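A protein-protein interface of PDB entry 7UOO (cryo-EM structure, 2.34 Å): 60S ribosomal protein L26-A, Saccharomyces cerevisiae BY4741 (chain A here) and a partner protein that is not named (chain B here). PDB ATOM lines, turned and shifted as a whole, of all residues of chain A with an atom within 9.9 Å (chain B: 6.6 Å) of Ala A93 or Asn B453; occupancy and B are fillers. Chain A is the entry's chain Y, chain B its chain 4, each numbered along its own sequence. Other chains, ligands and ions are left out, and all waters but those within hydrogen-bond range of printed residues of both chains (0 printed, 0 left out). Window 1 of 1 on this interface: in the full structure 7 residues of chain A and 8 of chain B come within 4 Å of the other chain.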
ATOM      1  N   ASP A  83     -31.844  12.605  14.888  1.00  0.00           N
ATOM      2  CA  ASP A  83     -31.240  12.001  16.074  1.00  0.00           C
ATOM      3  C   ASP A  83     -32.286  11.653  17.129  1.00  0.00           C
ATOM      4  O   ASP A  83     -32.188  10.610  17.787  1.00  0.00           O
ATOM      5  CB  ASP A  83     -30.176  12.936  16.652  1.00  0.00           C
ATOM      6  CG  ASP A  83     -30.640  14.378  16.732  1.00  0.00           C
ATOM      7  OD1 ASP A  83     -31.850  14.633  16.560  1.00  0.00           O
ATOM      8  OD2 ASP A  83     -29.788  15.264  16.959  1.00  0.00           O
ATOM      9  N   THR A  86     -36.271   7.688  16.730  1.00  0.00           N
ATOM     10  CA  THR A  86     -35.640   6.383  16.607  1.00  0.00           C
ATOM     11  C   THR A  86     -36.619   5.299  17.043  1.00  0.00           C
ATOM     12  O   THR A  86     -37.745   5.575  17.465  1.00  0.00           O
ATOM     13  CB  THR A  86     -34.353   6.310  17.437  1.00  0.00           C
ATOM     14  OG1 THR A  86     -34.655   6.565  18.814  1.00  0.00           O
ATOM     15  CG2 THR A  86     -33.329   7.317  16.952  1.00  0.00           C
ATOM     16  N   LYS A  87     -36.171   4.053  16.932  1.00  0.00           N
ATOM     17  CA  LYS A  87     -36.899   2.884  17.403  1.00  0.00           C
ATOM     18  C   LYS A  87     -35.991   2.113  18.350  1.00  0.00           C
ATOM     19  O   LYS A  87     -34.824   1.871  18.031  1.00  0.00           O
ATOM     20  CB  LYS A  87     -37.336   2.009  16.225  1.00  0.00           C
ATOM     21  CG  LYS A  87     -38.245   0.851  16.586  1.00  0.00           C
ATOM     22  CD  LYS A  87     -38.820   0.210  15.333  1.00  0.00           C
ATOM     23  CE  LYS A  87     -39.705  -0.979  15.670  1.00  0.00           C
ATOM     24  NZ  LYS A  87     -38.933  -2.083  16.298  1.00  0.00           N
ATOM     25  N   GLU A  88     -36.522   1.731  19.508  1.00  0.00           N
ATOM     26  CA  GLU A  88     -35.724   1.148  20.575  1.00  0.00           C
ATOM     27  C   GLU A  88     -36.098  -0.312  20.803  1.00  0.00           C
ATOM     28  O   GLU A  88     -37.259  -0.703  20.664  1.00  0.00           O
ATOM     29  CB  GLU A  88     -35.900   1.926  21.881  1.00  0.00           C
ATOM     30  CG  GLU A  88     -35.379   3.354  21.835  1.00  0.00           C
ATOM     31  CD  GLU A  88     -36.385   4.336  21.272  1.00  0.00           C
ATOM     32  OE1 GLU A  88     -37.481   3.906  20.858  1.00  0.00           O
ATOM     33  OE2 GLU A  88     -36.079   5.545  21.242  1.00  0.00           O
ATOM     34  N   LYS A  89     -35.097  -1.111  21.155  1.00  0.00           N
ATOM     35  CA  LYS A  89     -35.284  -2.513  21.502  1.00  0.00           C
ATOM     36  C   LYS A  89     -34.942  -2.731  22.971  1.00  0.00           C
ATOM     37  O   LYS A  89     -34.433  -1.841  23.655  1.00  0.00           O
ATOM     38  CB  LYS A  89     -34.427  -3.424  20.613  1.00  0.00           C
ATOM     39  CG  LYS A  89     -34.653  -3.246  19.122  1.00  0.00           C
ATOM     40  CD  LYS A  89     -33.790  -4.211  18.325  1.00  0.00           C
ATOM     41  CE  LYS A  89     -33.781  -3.862  16.850  1.00  0.00           C
ATOM     42  NZ  LYS A  89     -32.793  -4.668  16.087  1.00  0.00           N
ATOM     43  N   VAL A  90     -35.239  -3.942  23.451  1.00  0.00           N
ATOM     44  CA  VAL A  90     -34.965  -4.290  24.843  1.00  0.00           C
ATOM     45  C   VAL A  90     -33.464  -4.337  25.105  1.00  0.00           C
ATOM     46  O   VAL A  90     -32.986  -3.865  26.144  1.00  0.00           O
ATOM     47  CB  VAL A  90     -35.650  -5.622  25.200  1.00  0.00           C
ATOM     48  CG1 VAL A  90     -35.261  -6.077  26.599  1.00  0.00           C
ATOM     49  CG2 VAL A  90     -37.156  -5.488  25.088  1.00  0.00           C
ATOM     50  N   ASN A  91     -32.691  -4.878  24.164  1.00  0.00           N
ATOM     51  CA  ASN A  91     -31.256  -5.060  24.342  1.00  0.00           C
ATOM     52  C   ASN A  91     -30.456  -3.764  24.216  1.00  0.00           C
ATOM     53  O   ASN A  91     -29.225  -3.823  24.136  1.00  0.00           O
ATOM     54  CB  ASN A  91     -30.726  -6.095  23.345  1.00  0.00           C
ATOM     55  CG  ASN A  91     -31.055  -5.753  21.900  1.00  0.00           C
ATOM     56  OD1 ASN A  91     -31.480  -4.645  21.586  1.00  0.00           O
ATOM     57  ND2 ASN A  91     -30.859  -6.717  21.010  1.00  0.00           N
ATOM     58  N   GLY A  92     -31.113  -2.607  24.190  1.00  0.00           N
ATOM     59  CA  GLY A  92     -30.430  -1.341  24.056  1.00  0.00           C
ATOM     60  C   GLY A  92     -30.207  -0.878  22.635  1.00  0.00           C
ATOM     61  O   GLY A  92     -29.602   0.181  22.436  1.00  0.00           O
ATOM     62  N   ALA A  93     -30.667  -1.634  21.644  1.00  0.00           N
ATOM     63  CA  ALA A  93     -30.476  -1.238  20.258  1.00  0.00           C
ATOM     64  C   ALA A  93     -31.378  -0.062  19.897  1.00  0.00           C
ATOM     65  O   ALA A  93     -32.552  -0.015  20.275  1.00  0.00           O
ATOM     66  CB  ALA A  93     -30.749  -2.415  19.325  1.00  0.00           C
ATOM     67  N   SER A  94     -30.813   0.896  19.167  1.00  0.00           N
ATOM     68  CA  SER A  94     -31.556   2.034  18.643  1.00  0.00           C
ATOM     69  C   SER A  94     -31.351   2.089  17.139  1.00  0.00           C
ATOM     70  O   SER A  94     -30.212   2.168  16.668  1.00  0.00           O
ATOM     71  CB  SER A  94     -31.105   3.342  19.298  1.00  0.00           C
ATOM     72  OG  SER A  94     -31.387   3.334  20.685  1.00  0.00           O
ATOM     73  N   VAL A  95     -32.444   2.048  16.395  1.00  0.00           N
ATOM     74  CA  VAL A  95     -32.428   2.065  14.934  1.00  0.00           C
ATOM     75  C   VAL A  95     -33.041   3.380  14.472  1.00  0.00           C
ATOM     76  O   VAL A  95     -34.146   3.719  14.908  1.00  0.00           O
ATOM     77  CB  VAL A  95     -33.197   0.870  14.340  1.00  0.00           C
ATOM     78  CG1 VAL A  95     -33.090   0.866  12.826  1.00  0.00           C
ATOM     79  CG2 VAL A  95     -32.674  -0.436  14.917  1.00  0.00           C
ATOM     80  N   PRO A  96     -32.364   4.152  13.624  1.00  0.00           N
ATOM     81  CA  PRO A  96     -32.943   5.420  13.159  1.00  0.00           C
ATOM     82  C   PRO A  96     -34.169   5.198  12.286  1.00  0.00           C
ATOM     83  O   PRO A  96     -34.250   4.229  11.527  1.00  0.00           O
ATOM     84  CB  PRO A  96     -31.801   6.062  12.363  1.00  0.00           C
ATOM     85  CG  PRO A  96     -30.563   5.357  12.816  1.00  0.00           C
ATOM     86  CD  PRO A  96     -30.986   3.965  13.144  1.00  0.00           C
ATOM     87  N   ALA B 451     -26.315   9.271  20.071  1.00  0.00           N
ATOM     88  CA  ALA B 451     -25.868   8.231  19.161  1.00  0.00           C
ATOM     89  C   ALA B 451     -26.851   7.063  19.123  1.00  0.00           C
ATOM     90  O   ALA B 451     -27.629   6.832  20.052  1.00  0.00           O
ATOM     91  CB  ALA B 451     -24.489   7.727  19.567  1.00  0.00           C
ATOM     92  N   THR B 452     -26.801   6.318  18.021  1.00  0.00           N
ATOM     93  CA  THR B 452     -27.621   5.133  17.816  1.00  0.00           C
ATOM     94  C   THR B 452     -26.727   3.924  17.576  1.00  0.00           C
ATOM     95  O   THR B 452     -25.748   4.007  16.828  1.00  0.00           O
ATOM     96  CB  THR B 452     -28.567   5.309  16.625  1.00  0.00           C
ATOM     97  OG1 THR B 452     -27.799   5.468  15.425  1.00  0.00           O
ATOM     98  CG2 THR B 452     -29.456   6.528  16.820  1.00  0.00           C
ATOM     99  N   ASN B 453     -27.060   2.807  18.212  1.00  0.00           N
ATOM    100  CA  ASN B 453     -26.375   1.539  17.960  1.00  0.00           C
ATOM    101  C   ASN B 453     -27.395   0.492  17.538  1.00  0.00           C
ATOM    102  O   ASN B 453     -28.214   0.058  18.370  1.00  0.00           O
ATOM    103  CB  ASN B 453     -25.590   1.074  19.188  1.00  0.00           C
ATOM    104  CG  ASN B 453     -26.376   1.202  20.473  1.00  0.00           C
ATOM    105  OD1 ASN B 453     -27.272   2.037  20.586  1.00  0.00           O
ATOM    106  ND2 ASN B 453     -26.042   0.374  21.454  1.00  0.00           N
ATOM    107  N   PRO B 454     -27.406   0.073  16.269  1.00  0.00           N
ATOM    108  CA  PRO B 454     -28.430  -0.883  15.814  1.00  0.00           C
ATOM    109  C   PRO B 454     -28.336  -2.256  16.458  1.00  0.00           C
ATOM    110  O   PRO B 454     -29.324  -2.998  16.422  1.00  0.00           O
ATOM    111  CB  PRO B 454     -28.186  -0.964  14.300  1.00  0.00           C
ATOM    112  CG  PRO B 454     -27.444   0.286  13.963  1.00  0.00           C
ATOM    113  CD  PRO B 454     -26.586   0.573  15.155  1.00  0.00           C
ATOM    114  N   ASN B 455     -27.197  -2.622  17.039  1.00  0.00           N
ATOM    115  CA  ASN B 455     -27.014  -3.948  17.619  1.00  0.00           C
ATOM    116  C   ASN B 455     -27.209  -3.979  19.128  1.00  0.00           C
ATOM    117  O   ASN B 455     -27.726  -4.969  19.657  1.00  0.00           O
ATOM    118  CB  ASN B 455     -25.622  -4.485  17.271  1.00  0.00           C
ATOM    119  CG  ASN B 455     -25.481  -4.825  15.802  1.00  0.00           C
ATOM    120  OD1 ASN B 455     -26.343  -5.486  15.222  1.00  0.00           O
ATOM    121  ND2 ASN B 455     -24.395  -4.372  15.189  1.00  0.00           N
ATOM    122  N   GLY B 456     -26.813  -2.926  19.839  1.00  0.00           N
ATOM    123  CA  GLY B 456     -26.991  -2.878  21.277  1.00  0.00           C
ATOM    124  C   GLY B 456     -26.023  -3.753  22.050  1.00  0.00           C
ATOM    125  O   GLY B 456     -24.805  -3.600  21.926  1.00  0.00           O
ATOM    126  N   ASN B 457     -26.561  -4.673  22.854  1.00  0.00           N
ATOM    127  CA  ASN B 457     -25.722  -5.557  23.660  1.00  0.00           C
ATOM    128  C   ASN B 457     -24.969  -6.575  22.813  1.00  0.00           C
ATOM    129  O   ASN B 457     -23.921  -7.073  23.238  1.00  0.00           O
ATOM    130  CB  ASN B 457     -26.573  -6.296  24.691  1.00  0.00           C
ATOM    131  CG  ASN B 457     -26.920  -5.440  25.882  1.00  0.00           C
ATOM    132  OD1 ASN B 457     -26.200  -4.501  26.215  1.00  0.00           O
ATOM    133  ND2 ASN B 457     -28.025  -5.765  26.540  1.00  0.00           N
ATOM    134  N   SER B 459     -23.286  -6.490  19.995  1.00  0.00           N
ATOM    135  CA  SER B 459     -22.054  -6.154  19.294  1.00  0.00           C
ATOM    136  C   SER B 459     -20.833  -6.317  20.195  1.00  0.00           C
ATOM    137  O   SER B 459     -20.893  -6.106  21.408  1.00  0.00           O
ATOM    138  CB  SER B 459     -22.124  -4.726  18.756  1.00  0.00           C
ATOM    139  OG  SER B 459     -22.429  -3.809  19.788  1.00  0.00           O
ATOM    140  N   LEU B 478     -27.136   1.373  29.206  1.00  0.00           N
ATOM    141  CA  LEU B 478     -27.426   1.910  27.885  1.00  0.00           C
ATOM    142  C   LEU B 478     -27.223   0.886  26.777  1.00  0.00           C
ATOM    143  O   LEU B 478     -27.630   1.142  25.639  1.00  0.00           O
ATOM    144  CB  LEU B 478     -26.556   3.138  27.610  1.00  0.00           C
ATOM    145  CG  LEU B 478     -26.866   4.397  28.422  1.00  0.00           C
ATOM    146  CD1 LEU B 478     -25.716   5.387  28.335  1.00  0.00           C
ATOM    147  CD2 LEU B 478     -28.158   5.035  27.942  1.00  0.00           C
ATOM    148  N   GLY B 479     -26.619  -0.258  27.079  1.00  0.00           N
ATOM    149  CA  GLY B 479     -26.341  -1.260  26.066  1.00  0.00           C
ATOM    150  C   GLY B 479     -25.326  -0.831  25.030  1.00  0.00           C
ATOM    151  O   GLY B 479     -25.523  -1.086  23.835  1.00  0.00           O
ATOM    152  N   VAL B 480     -24.247  -0.181  25.454  1.00  0.00           N
ATOM    153  CA  VAL B 480     -23.206   0.305  24.556  1.00  0.00           C
ATOM    154  C   VAL B 480     -21.961  -0.541  24.773  1.00  0.00           C
ATOM    155  O   VAL B 480     -21.438  -0.615  25.891  1.00  0.00           O
ATOM    156  CB  VAL B 480     -22.908   1.795  24.782  1.00  0.00           C
ATOM    157  CG1 VAL B 480     -21.858   2.280  23.793  1.00  0.00           C
ATOM    158  CG2 VAL B 480     -24.180   2.616  24.666  1.00  0.00           C
ATOM    159  N   SER B 481     -21.483  -1.169  23.705  1.00  0.00           N
ATOM    160  CA  SER B 481     -20.313  -2.028  23.765  1.00  0.00           C
ATOM    161  C   SER B 481     -19.031  -1.210  23.614  1.00  0.00           C
ATOM    162  O   SER B 481     -19.055  -0.005  23.365  1.00  0.00           O
ATOM    163  CB  SER B 481     -20.392  -3.106  22.686  1.00  0.00           C
ATOM    164  OG  SER B 481     -20.480  -2.529  21.395  1.00  0.00           O
ATOM    165  N   LYS B 484     -18.578   0.063  19.997  1.00  0.00           N
ATOM    166  CA  LYS B 484     -19.441   1.222  19.795  1.00  0.00           C
ATOM    167  C   LYS B 484     -18.897   2.447  20.520  1.00  0.00           C
ATOM    168  O   LYS B 484     -18.968   3.563  19.997  1.00  0.00           O
ATOM    169  CB  LYS B 484     -20.864   0.910  20.257  1.00  0.00           C
ATOM    170  CG  LYS B 484     -21.869   1.996  19.916  1.00  0.00           C
ATOM    171  CD  LYS B 484     -21.853   2.306  18.428  1.00  0.00           C
ATOM    172  CE  LYS B 484     -22.780   3.457  18.091  1.00  0.00           C
ATOM    173  NZ  LYS B 484     -22.693   3.837  16.654  1.00  0.00           N
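The backbone carbonyl oxygen (O) of Asn A91 is in hydrogen-bond range of the backbone NH (N) of Asn B457 (3.1 Å). O of Asn B453 sits at hydrogen-bond distance from N of Ser A94, at 2.8 Å.
The side-chain carboxylate (OE2) of Glu A88 is in hydrogen-bond range of the side-chain hydroxyl (OG1) of Thr A86 (3.0 Å). The backbone NH (N) of Ala A93 lies within hydrogen-bond range of the side-chain amide oxygen (OD1) of Asn A91. O of Thr B452 lies within hydrogen-bond range of NZ of Lys B484. O of Gly B479 lies within hydrogen-bond range of ND2 of Asn B453 (2.8 Å). The backbone carbonyl oxygen (O) of Gly B456 lies within hydrogen-bond range of the side-chain hydroxyl (OG) of Ser B459, at 3.2 Å.
Thr B452 touches Thr A86. ND2 of Asn A91 touches O of Asn B455, at 3.8 Å. Asn A91 touches Gly B456. Asn B453 touches Gly A92 (OD1 to O, 3.5 Å). Gly A92 touches Leu B478. CB of Ala A93 touches O of Pro B454 (3.3 Å). Ala A93 touches Asn B455. Ala A93 touches Gly B456 (N to CA, 3.9 Å). Ser A94 touches Thr B452 (O to CB, 3.5 Å). CG of Pro A96 touches OG1 of Thr B452, at 3.8 Å.
Asn B453 touches just these residues of chain A: Gly A92 (3.5 Å), Ala A93 (3.2 Å) and Ser A94 (2.8 Å). Of chain A, only Thr A86, Ser A94 and Pro A96 come within 4 Å of Thr B452. No residue of chain A comes within 4 Å of Gly B479. Printed residues of chain A within 4 Å of Asn B457: Asn A91 (3.1 Å). Of the printed residues of chain B, Asn A91 touches Asn B455, Gly B456 and Asn B457. Of the printed residues of chain B, Gly A92 touches Asn B453 and Leu B478. Of the printed residues of chain B, Lys A89 touches Pro B454. Printed residues of chain A within 4 Å of Leu B478: Gly A92. The nearest printed residue of chain B that does not touch Asn A91 is Gly B479 (4.3 Å).
Along chain A the printed residues that touch a printed residue of chain B span positions 86 to 96. Of the 13 printed residues of chain B, 7 touch a printed residue of chain A. Among the printed residues, 15 pairs touch across the chains. Among the printed residues, no Asp or Glu carboxylate lies within 4 Å of a Lys or Arg side-chain nitrogen of the other chain.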
